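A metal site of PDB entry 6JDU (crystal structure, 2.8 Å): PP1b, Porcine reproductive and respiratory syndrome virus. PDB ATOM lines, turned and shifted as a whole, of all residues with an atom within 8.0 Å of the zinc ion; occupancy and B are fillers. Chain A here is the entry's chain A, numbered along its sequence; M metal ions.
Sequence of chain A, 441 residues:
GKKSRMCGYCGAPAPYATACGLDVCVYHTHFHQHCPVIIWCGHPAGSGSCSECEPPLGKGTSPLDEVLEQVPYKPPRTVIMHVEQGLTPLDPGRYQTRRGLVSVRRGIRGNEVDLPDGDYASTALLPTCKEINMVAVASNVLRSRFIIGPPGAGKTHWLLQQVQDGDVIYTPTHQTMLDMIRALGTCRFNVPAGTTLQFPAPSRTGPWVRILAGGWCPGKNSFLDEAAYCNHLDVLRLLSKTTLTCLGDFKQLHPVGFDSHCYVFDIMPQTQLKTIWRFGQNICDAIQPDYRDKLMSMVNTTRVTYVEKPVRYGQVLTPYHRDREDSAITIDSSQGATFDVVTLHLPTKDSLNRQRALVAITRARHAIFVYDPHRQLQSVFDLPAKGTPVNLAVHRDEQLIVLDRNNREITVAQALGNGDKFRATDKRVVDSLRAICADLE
ND1 of His 32 lies within hydrogen-bond range of OH of Tyr 9 (2.6 Å). NE2 of His 34 sits at hydrogen-bond distance from O of Val 71 (2.8 Å). The side-chain sulfur (SG) of Cys 35 sits close to the backbone NH (N) of Ala 19. The backbone NH (N) of Cys 20 lies close to the side-chain hydroxyl (OG1) of Thr 18 (3.4 Å). O of Cys 20 lies within hydrogen-bond range of N of Cys 129 (2.7 Å). OG1 of Thr 18 sits at hydrogen-bond distance from N of Gly 21 (3.3 Å). The side-chain hydroxyl of Thr 18 lies within hydrogen-bond range of the backbone NH of Leu 22, at 2.9 Å.
The zinc ion is bound by a ring nitrogen (NE2) of His 32 (2.0 Å), a ring nitrogen (ND1) of His 34 (2.0 Å), the side-chain sulfur of Cys 35 (2.1 Å) and the side-chain sulfur of Cys 20 (2.2 Å).
Thr 18 touches the zinc ion. Of the 21 residues printed, 5 come within 4 Å of the zinc ion. The nearest printed residue that does not touch the zinc ion is Leu 68 (4.4 Å).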
ATOM      1  N   TYR A   9     -25.804  -8.601  -4.658  1.00  0.00           N
ATOM      2  CA  TYR A   9     -27.016  -8.914  -3.897  1.00  0.00           C
ATOM      3  C   TYR A   9     -28.085  -9.540  -4.798  1.00  0.00           C
ATOM      4  O   TYR A   9     -28.485 -10.688  -4.604  1.00  0.00           O
ATOM      5  CB  TYR A   9     -27.593  -7.657  -3.226  1.00  0.00           C
ATOM      6  CG  TYR A   9     -26.687  -6.977  -2.235  1.00  0.00           C
ATOM      7  CD1 TYR A   9     -26.440  -7.556  -0.979  1.00  0.00           C
ATOM      8  CD2 TYR A   9     -26.098  -5.750  -2.509  1.00  0.00           C
ATOM      9  CE1 TYR A   9     -25.618  -6.937  -0.052  1.00  0.00           C
ATOM     10  CE2 TYR A   9     -25.283  -5.116  -1.587  1.00  0.00           C
ATOM     11  CZ  TYR A   9     -25.044  -5.715  -0.353  1.00  0.00           C
ATOM     12  OH  TYR A   9     -24.238  -5.088   0.560  1.00  0.00           O
ATOM     13  N   ALA A  17     -19.310  -0.396  -7.412  1.00  0.00           N
ATOM     14  CA  ALA A  17     -18.771  -1.409  -6.513  1.00  0.00           C
ATOM     15  C   ALA A  17     -18.522  -0.848  -5.111  1.00  0.00           C
ATOM     16  O   ALA A  17     -18.347   0.363  -4.932  1.00  0.00           O
ATOM     17  CB  ALA A  17     -17.475  -1.974  -7.081  1.00  0.00           C
ATOM     18  N   THR A  18     -18.504  -1.726  -4.117  1.00  0.00           N
ATOM     19  CA  THR A  18     -18.151  -1.354  -2.750  1.00  0.00           C
ATOM     20  C   THR A  18     -16.639  -1.292  -2.658  1.00  0.00           C
ATOM     21  O   THR A  18     -15.932  -1.815  -3.527  1.00  0.00           O
ATOM     22  CB  THR A  18     -18.686  -2.375  -1.732  1.00  0.00           C
ATOM     23  OG1 THR A  18     -18.056  -3.651  -1.941  1.00  0.00           O
ATOM     24  CG2 THR A  18     -20.193  -2.540  -1.852  1.00  0.00           C
ATOM     25  N   ALA A  19     -16.125  -0.679  -1.595  1.00  0.00           N
ATOM     26  CA  ALA A  19     -14.677  -0.667  -1.346  1.00  0.00           C
ATOM     27  C   ALA A  19     -14.145  -2.075  -1.074  1.00  0.00           C
ATOM     28  O   ALA A  19     -12.992  -2.374  -1.355  1.00  0.00           O
ATOM     29  CB  ALA A  19     -14.330   0.249  -0.197  1.00  0.00           C
ATOM     30  N   CYS A  20     -15.027  -2.928  -0.538  1.00  0.00           N
ATOM     31  CA  CYS A  20     -14.704  -4.329  -0.253  1.00  0.00           C
ATOM     32  C   CYS A  20     -14.864  -5.321  -1.439  1.00  0.00           C
ATOM     33  O   CYS A  20     -14.813  -6.519  -1.238  1.00  0.00           O
ATOM     34  CB  CYS A  20     -15.553  -4.788   0.944  1.00  0.00           C
ATOM     35  SG  CYS A  20     -17.323  -4.986   0.605  1.00  0.00           S
ATOM     36  N   GLY A  21     -15.067  -4.807  -2.655  1.00  0.00           N
ATOM     37  CA  GLY A  21     -15.051  -5.643  -3.874  1.00  0.00           C
ATOM     38  C   GLY A  21     -16.372  -6.224  -4.362  1.00  0.00           C
ATOM     39  O   GLY A  21     -16.392  -6.953  -5.357  1.00  0.00           O
ATOM     40  N   LEU A  22     -17.471  -5.913  -3.680  1.00  0.00           N
ATOM     41  CA  LEU A  22     -18.802  -6.352  -4.111  1.00  0.00           C
ATOM     42  C   LEU A  22     -19.345  -5.422  -5.193  1.00  0.00           C
ATOM     43  O   LEU A  22     -19.467  -4.214  -4.968  1.00  0.00           O
ATOM     44  CB  LEU A  22     -19.764  -6.359  -2.913  1.00  0.00           C
ATOM     45  CG  LEU A  22     -21.093  -7.069  -3.105  1.00  0.00           C
ATOM     46  CD1 LEU A  22     -20.912  -8.576  -3.062  1.00  0.00           C
ATOM     47  CD2 LEU A  22     -22.084  -6.639  -2.025  1.00  0.00           C
ATOM     48  N   HIS A  32     -25.308  -0.581   1.660  1.00  0.00           N
ATOM     49  CA  HIS A  32     -24.062  -1.248   2.045  1.00  0.00           C
ATOM     50  C   HIS A  32     -23.305  -0.368   3.035  1.00  0.00           C
ATOM     51  O   HIS A  32     -22.428   0.427   2.665  1.00  0.00           O
ATOM     52  CB  HIS A  32     -23.211  -1.568   0.796  1.00  0.00           C
ATOM     53  CG  HIS A  32     -22.013  -2.417   1.075  1.00  0.00           C
ATOM     54  ND1 HIS A  32     -22.028  -3.795   1.016  1.00  0.00           N
ATOM     55  CD2 HIS A  32     -20.734  -2.080   1.403  1.00  0.00           C
ATOM     56  CE1 HIS A  32     -20.836  -4.270   1.298  1.00  0.00           C
ATOM     57  NE2 HIS A  32     -20.029  -3.245   1.527  1.00  0.00           N
ATOM     58  N   GLN A  33     -23.660  -0.514   4.310  1.00  0.00           N
ATOM     59  CA  GLN A  33     -23.089   0.285   5.390  1.00  0.00           C
ATOM     60  C   GLN A  33     -21.693  -0.164   5.826  1.00  0.00           C
ATOM     61  O   GLN A  33     -20.981   0.579   6.501  1.00  0.00           O
ATOM     62  CB  GLN A  33     -24.009   0.269   6.614  1.00  0.00           C
ATOM     63  CG  GLN A  33     -25.407   0.805   6.342  1.00  0.00           C
ATOM     64  CD  GLN A  33     -26.202   1.030   7.609  1.00  0.00           C
ATOM     65  OE1 GLN A  33     -25.935   0.442   8.651  1.00  0.00           O
ATOM     66  NE2 GLN A  33     -27.206   1.900   7.520  1.00  0.00           N
ATOM     67  N   HIS A  34     -21.317  -1.395   5.460  1.00  0.00           N
ATOM     68  CA  HIS A  34     -20.016  -1.991   5.803  1.00  0.00           C
ATOM     69  C   HIS A  34     -18.816  -1.115   5.432  1.00  0.00           C
ATOM     70  O   HIS A  34     -17.914  -0.913   6.246  1.00  0.00           O
ATOM     71  CB  HIS A  34     -19.891  -3.365   5.132  1.00  0.00           C
ATOM     72  CG  HIS A  34     -18.510  -3.927   5.126  1.00  0.00           C
ATOM     73  ND1 HIS A  34     -17.699  -3.906   4.008  1.00  0.00           N
ATOM     74  CD2 HIS A  34     -17.776  -4.521   6.101  1.00  0.00           C
ATOM     75  CE1 HIS A  34     -16.532  -4.458   4.300  1.00  0.00           C
ATOM     76  NE2 HIS A  34     -16.558  -4.841   5.556  1.00  0.00           N
ATOM     77  N   CYS A  35     -18.838  -0.594   4.203  1.00  0.00           N
ATOM     78  CA  CYS A  35     -17.729   0.209   3.661  1.00  0.00           C
ATOM     79  C   CYS A  35     -18.252   1.221   2.637  1.00  0.00           C
ATOM     80  O   CYS A  35     -19.415   1.136   2.240  1.00  0.00           O
ATOM     81  CB  CYS A  35     -16.684  -0.724   3.025  1.00  0.00           C
ATOM     82  SG  CYS A  35     -17.307  -1.744   1.684  1.00  0.00           S
ATOM     83  N   PRO A  36     -17.421   2.194   2.224  1.00  0.00           N
ATOM     84  CA  PRO A  36     -17.906   3.188   1.249  1.00  0.00           C
ATOM     85  C   PRO A  36     -18.154   2.593  -0.137  1.00  0.00           C
ATOM     86  O   PRO A  36     -17.409   1.721  -0.566  1.00  0.00           O
ATOM     87  CB  PRO A  36     -16.758   4.216   1.178  1.00  0.00           C
ATOM     88  CG  PRO A  36     -15.914   3.959   2.377  1.00  0.00           C
ATOM     89  CD  PRO A  36     -16.039   2.505   2.650  1.00  0.00           C
ATOM     90  N   VAL A  37     -19.198   3.077  -0.807  1.00  0.00           N
ATOM     91  CA  VAL A  37     -19.434   2.778  -2.218  1.00  0.00           C
ATOM     92  C   VAL A  37     -19.495   4.116  -2.956  1.00  0.00           C
ATOM     93  O   VAL A  37     -20.423   4.904  -2.752  1.00  0.00           O
ATOM     94  CB  VAL A  37     -20.683   1.878  -2.468  1.00  0.00           C
ATOM     95  CG1 VAL A  37     -21.721   1.985  -1.354  1.00  0.00           C
ATOM     96  CG2 VAL A  37     -21.333   2.119  -3.839  1.00  0.00           C
ATOM     97  N   LEU A  64     -25.843 -11.215   3.729  1.00  0.00           N
ATOM     98  CA  LEU A  64     -24.475 -10.756   3.492  1.00  0.00           C
ATOM     99  C   LEU A  64     -24.090  -9.567   4.376  1.00  0.00           C
ATOM    100  O   LEU A  64     -22.996  -9.519   4.934  1.00  0.00           O
ATOM    101  CB  LEU A  64     -24.289 -10.386   2.012  1.00  0.00           C
ATOM    102  CG  LEU A  64     -22.944  -9.789   1.588  1.00  0.00           C
ATOM    103  CD1 LEU A  64     -21.780 -10.683   2.002  1.00  0.00           C
ATOM    104  CD2 LEU A  64     -22.939  -9.575   0.077  1.00  0.00           C
ATOM    105  N   ASP A  65     -25.012  -8.618   4.483  1.00  0.00           N
ATOM    106  CA  ASP A  65     -24.793  -7.415   5.281  1.00  0.00           C
ATOM    107  C   ASP A  65     -24.630  -7.762   6.752  1.00  0.00           C
ATOM    108  O   ASP A  65     -23.795  -7.182   7.432  1.00  0.00           O
ATOM    109  CB  ASP A  65     -25.952  -6.424   5.084  1.00  0.00           C
ATOM    110  CG  ASP A  65     -26.182  -6.076   3.627  1.00  0.00           C
ATOM    111  OD1 ASP A  65     -25.190  -5.759   2.938  1.00  0.00           O
ATOM    112  OD2 ASP A  65     -27.344  -6.130   3.168  1.00  0.00           O
ATOM    113  N   LEU A  68     -21.232  -9.347   7.233  1.00  0.00           N
ATOM    114  CA  LEU A  68     -20.252  -8.258   7.094  1.00  0.00           C
ATOM    115  C   LEU A  68     -20.104  -7.359   8.336  1.00  0.00           C
ATOM    116  O   LEU A  68     -19.119  -6.623   8.434  1.00  0.00           O
ATOM    117  CB  LEU A  68     -20.543  -7.410   5.830  1.00  0.00           C
ATOM    118  CG  LEU A  68     -19.682  -7.634   4.571  1.00  0.00           C
ATOM    119  CD1 LEU A  68     -19.171  -9.051   4.375  1.00  0.00           C
ATOM    120  CD2 LEU A  68     -20.435  -7.166   3.327  1.00  0.00           C
ATOM    121  N   VAL A  71     -16.830  -8.264   9.847  1.00  0.00           N
ATOM    122  CA  VAL A  71     -15.729  -8.227   8.893  1.00  0.00           C
ATOM    123  C   VAL A  71     -15.242  -6.772   8.798  1.00  0.00           C
ATOM    124  O   VAL A  71     -15.774  -6.006   7.989  1.00  0.00           O
ATOM    125  CB  VAL A  71     -16.178  -8.743   7.507  1.00  0.00           C
ATOM    126  CG1 VAL A  71     -14.999  -8.736   6.519  1.00  0.00           C
ATOM    127  CG2 VAL A  71     -16.782 -10.137   7.622  1.00  0.00           C
ATOM    128  N   TYR A  73     -13.673  -3.224   8.018  1.00  0.00           N
ATOM    129  CA  TYR A  73     -13.125  -2.577   6.821  1.00  0.00           C
ATOM    130  C   TYR A  73     -11.956  -1.666   7.178  1.00  0.00           C
ATOM    131  O   TYR A  73     -12.142  -0.643   7.830  1.00  0.00           O
ATOM    132  CB  TYR A  73     -14.199  -1.754   6.094  1.00  0.00           C
ATOM    133  CG  TYR A  73     -13.627  -0.903   4.983  1.00  0.00           C
ATOM    134  CD1 TYR A  73     -13.173  -1.478   3.802  1.00  0.00           C
ATOM    135  CD2 TYR A  73     -13.502   0.490   5.133  1.00  0.00           C
ATOM    136  CE1 TYR A  73     -12.627  -0.710   2.786  1.00  0.00           C
ATOM    137  CE2 TYR A  73     -12.947   1.265   4.125  1.00  0.00           C
ATOM    138  CZ  TYR A  73     -12.512   0.666   2.958  1.00  0.00           C
ATOM    139  OH  TYR A  73     -11.971   1.437   1.955  1.00  0.00           O
ATOM    140  N   LEU A 126     -10.704  -4.088  -2.182  1.00  0.00           N
ATOM    141  CA  LEU A 126     -10.222  -5.211  -1.386  1.00  0.00           C
ATOM    142  C   LEU A 126     -10.775  -6.516  -1.966  1.00  0.00           C
ATOM    143  O   LEU A 126     -11.769  -6.499  -2.703  1.00  0.00           O
ATOM    144  CB  LEU A 126     -10.668  -5.057   0.064  1.00  0.00           C
ATOM    145  CG  LEU A 126     -10.298  -3.775   0.806  1.00  0.00           C
ATOM    146  CD1 LEU A 126     -10.841  -3.819   2.219  1.00  0.00           C
ATOM    147  CD2 LEU A 126      -8.790  -3.569   0.824  1.00  0.00           C
ATOM    148  N   THR A 128     -12.202  -8.833  -0.130  1.00  0.00           N
ATOM    149  CA  THR A 128     -13.247  -9.280   0.808  1.00  0.00           C
ATOM    150  C   THR A 128     -14.459  -9.924   0.151  1.00  0.00           C
ATOM    151  O   THR A 128     -14.754 -11.089   0.411  1.00  0.00           O
ATOM    152  CB  THR A 128     -13.751  -8.108   1.687  1.00  0.00           C
ATOM    153  OG1 THR A 128     -12.639  -7.492   2.344  1.00  0.00           O
ATOM    154  CG2 THR A 128     -14.748  -8.587   2.741  1.00  0.00           C
ATOM    155  N   CYS A 129     -15.164  -9.172  -0.703  1.00  0.00           N
ATOM    156  CA  CYS A 129     -16.364  -9.666  -1.374  1.00  0.00           C
ATOM    157  C   CYS A 129     -16.159  -9.879  -2.883  1.00  0.00           C
ATOM    158  O   CYS A 129     -17.112  -9.818  -3.661  1.00  0.00           O
ATOM    159  CB  CYS A 129     -17.528  -8.699  -1.120  1.00  0.00           C
ATOM    160  SG  CYS A 129     -18.109  -8.710   0.603  1.00  0.00           S
HETATM  161 ZN    ZN M   1     -18.161  -3.573   2.054  1.00  0.00          ZN
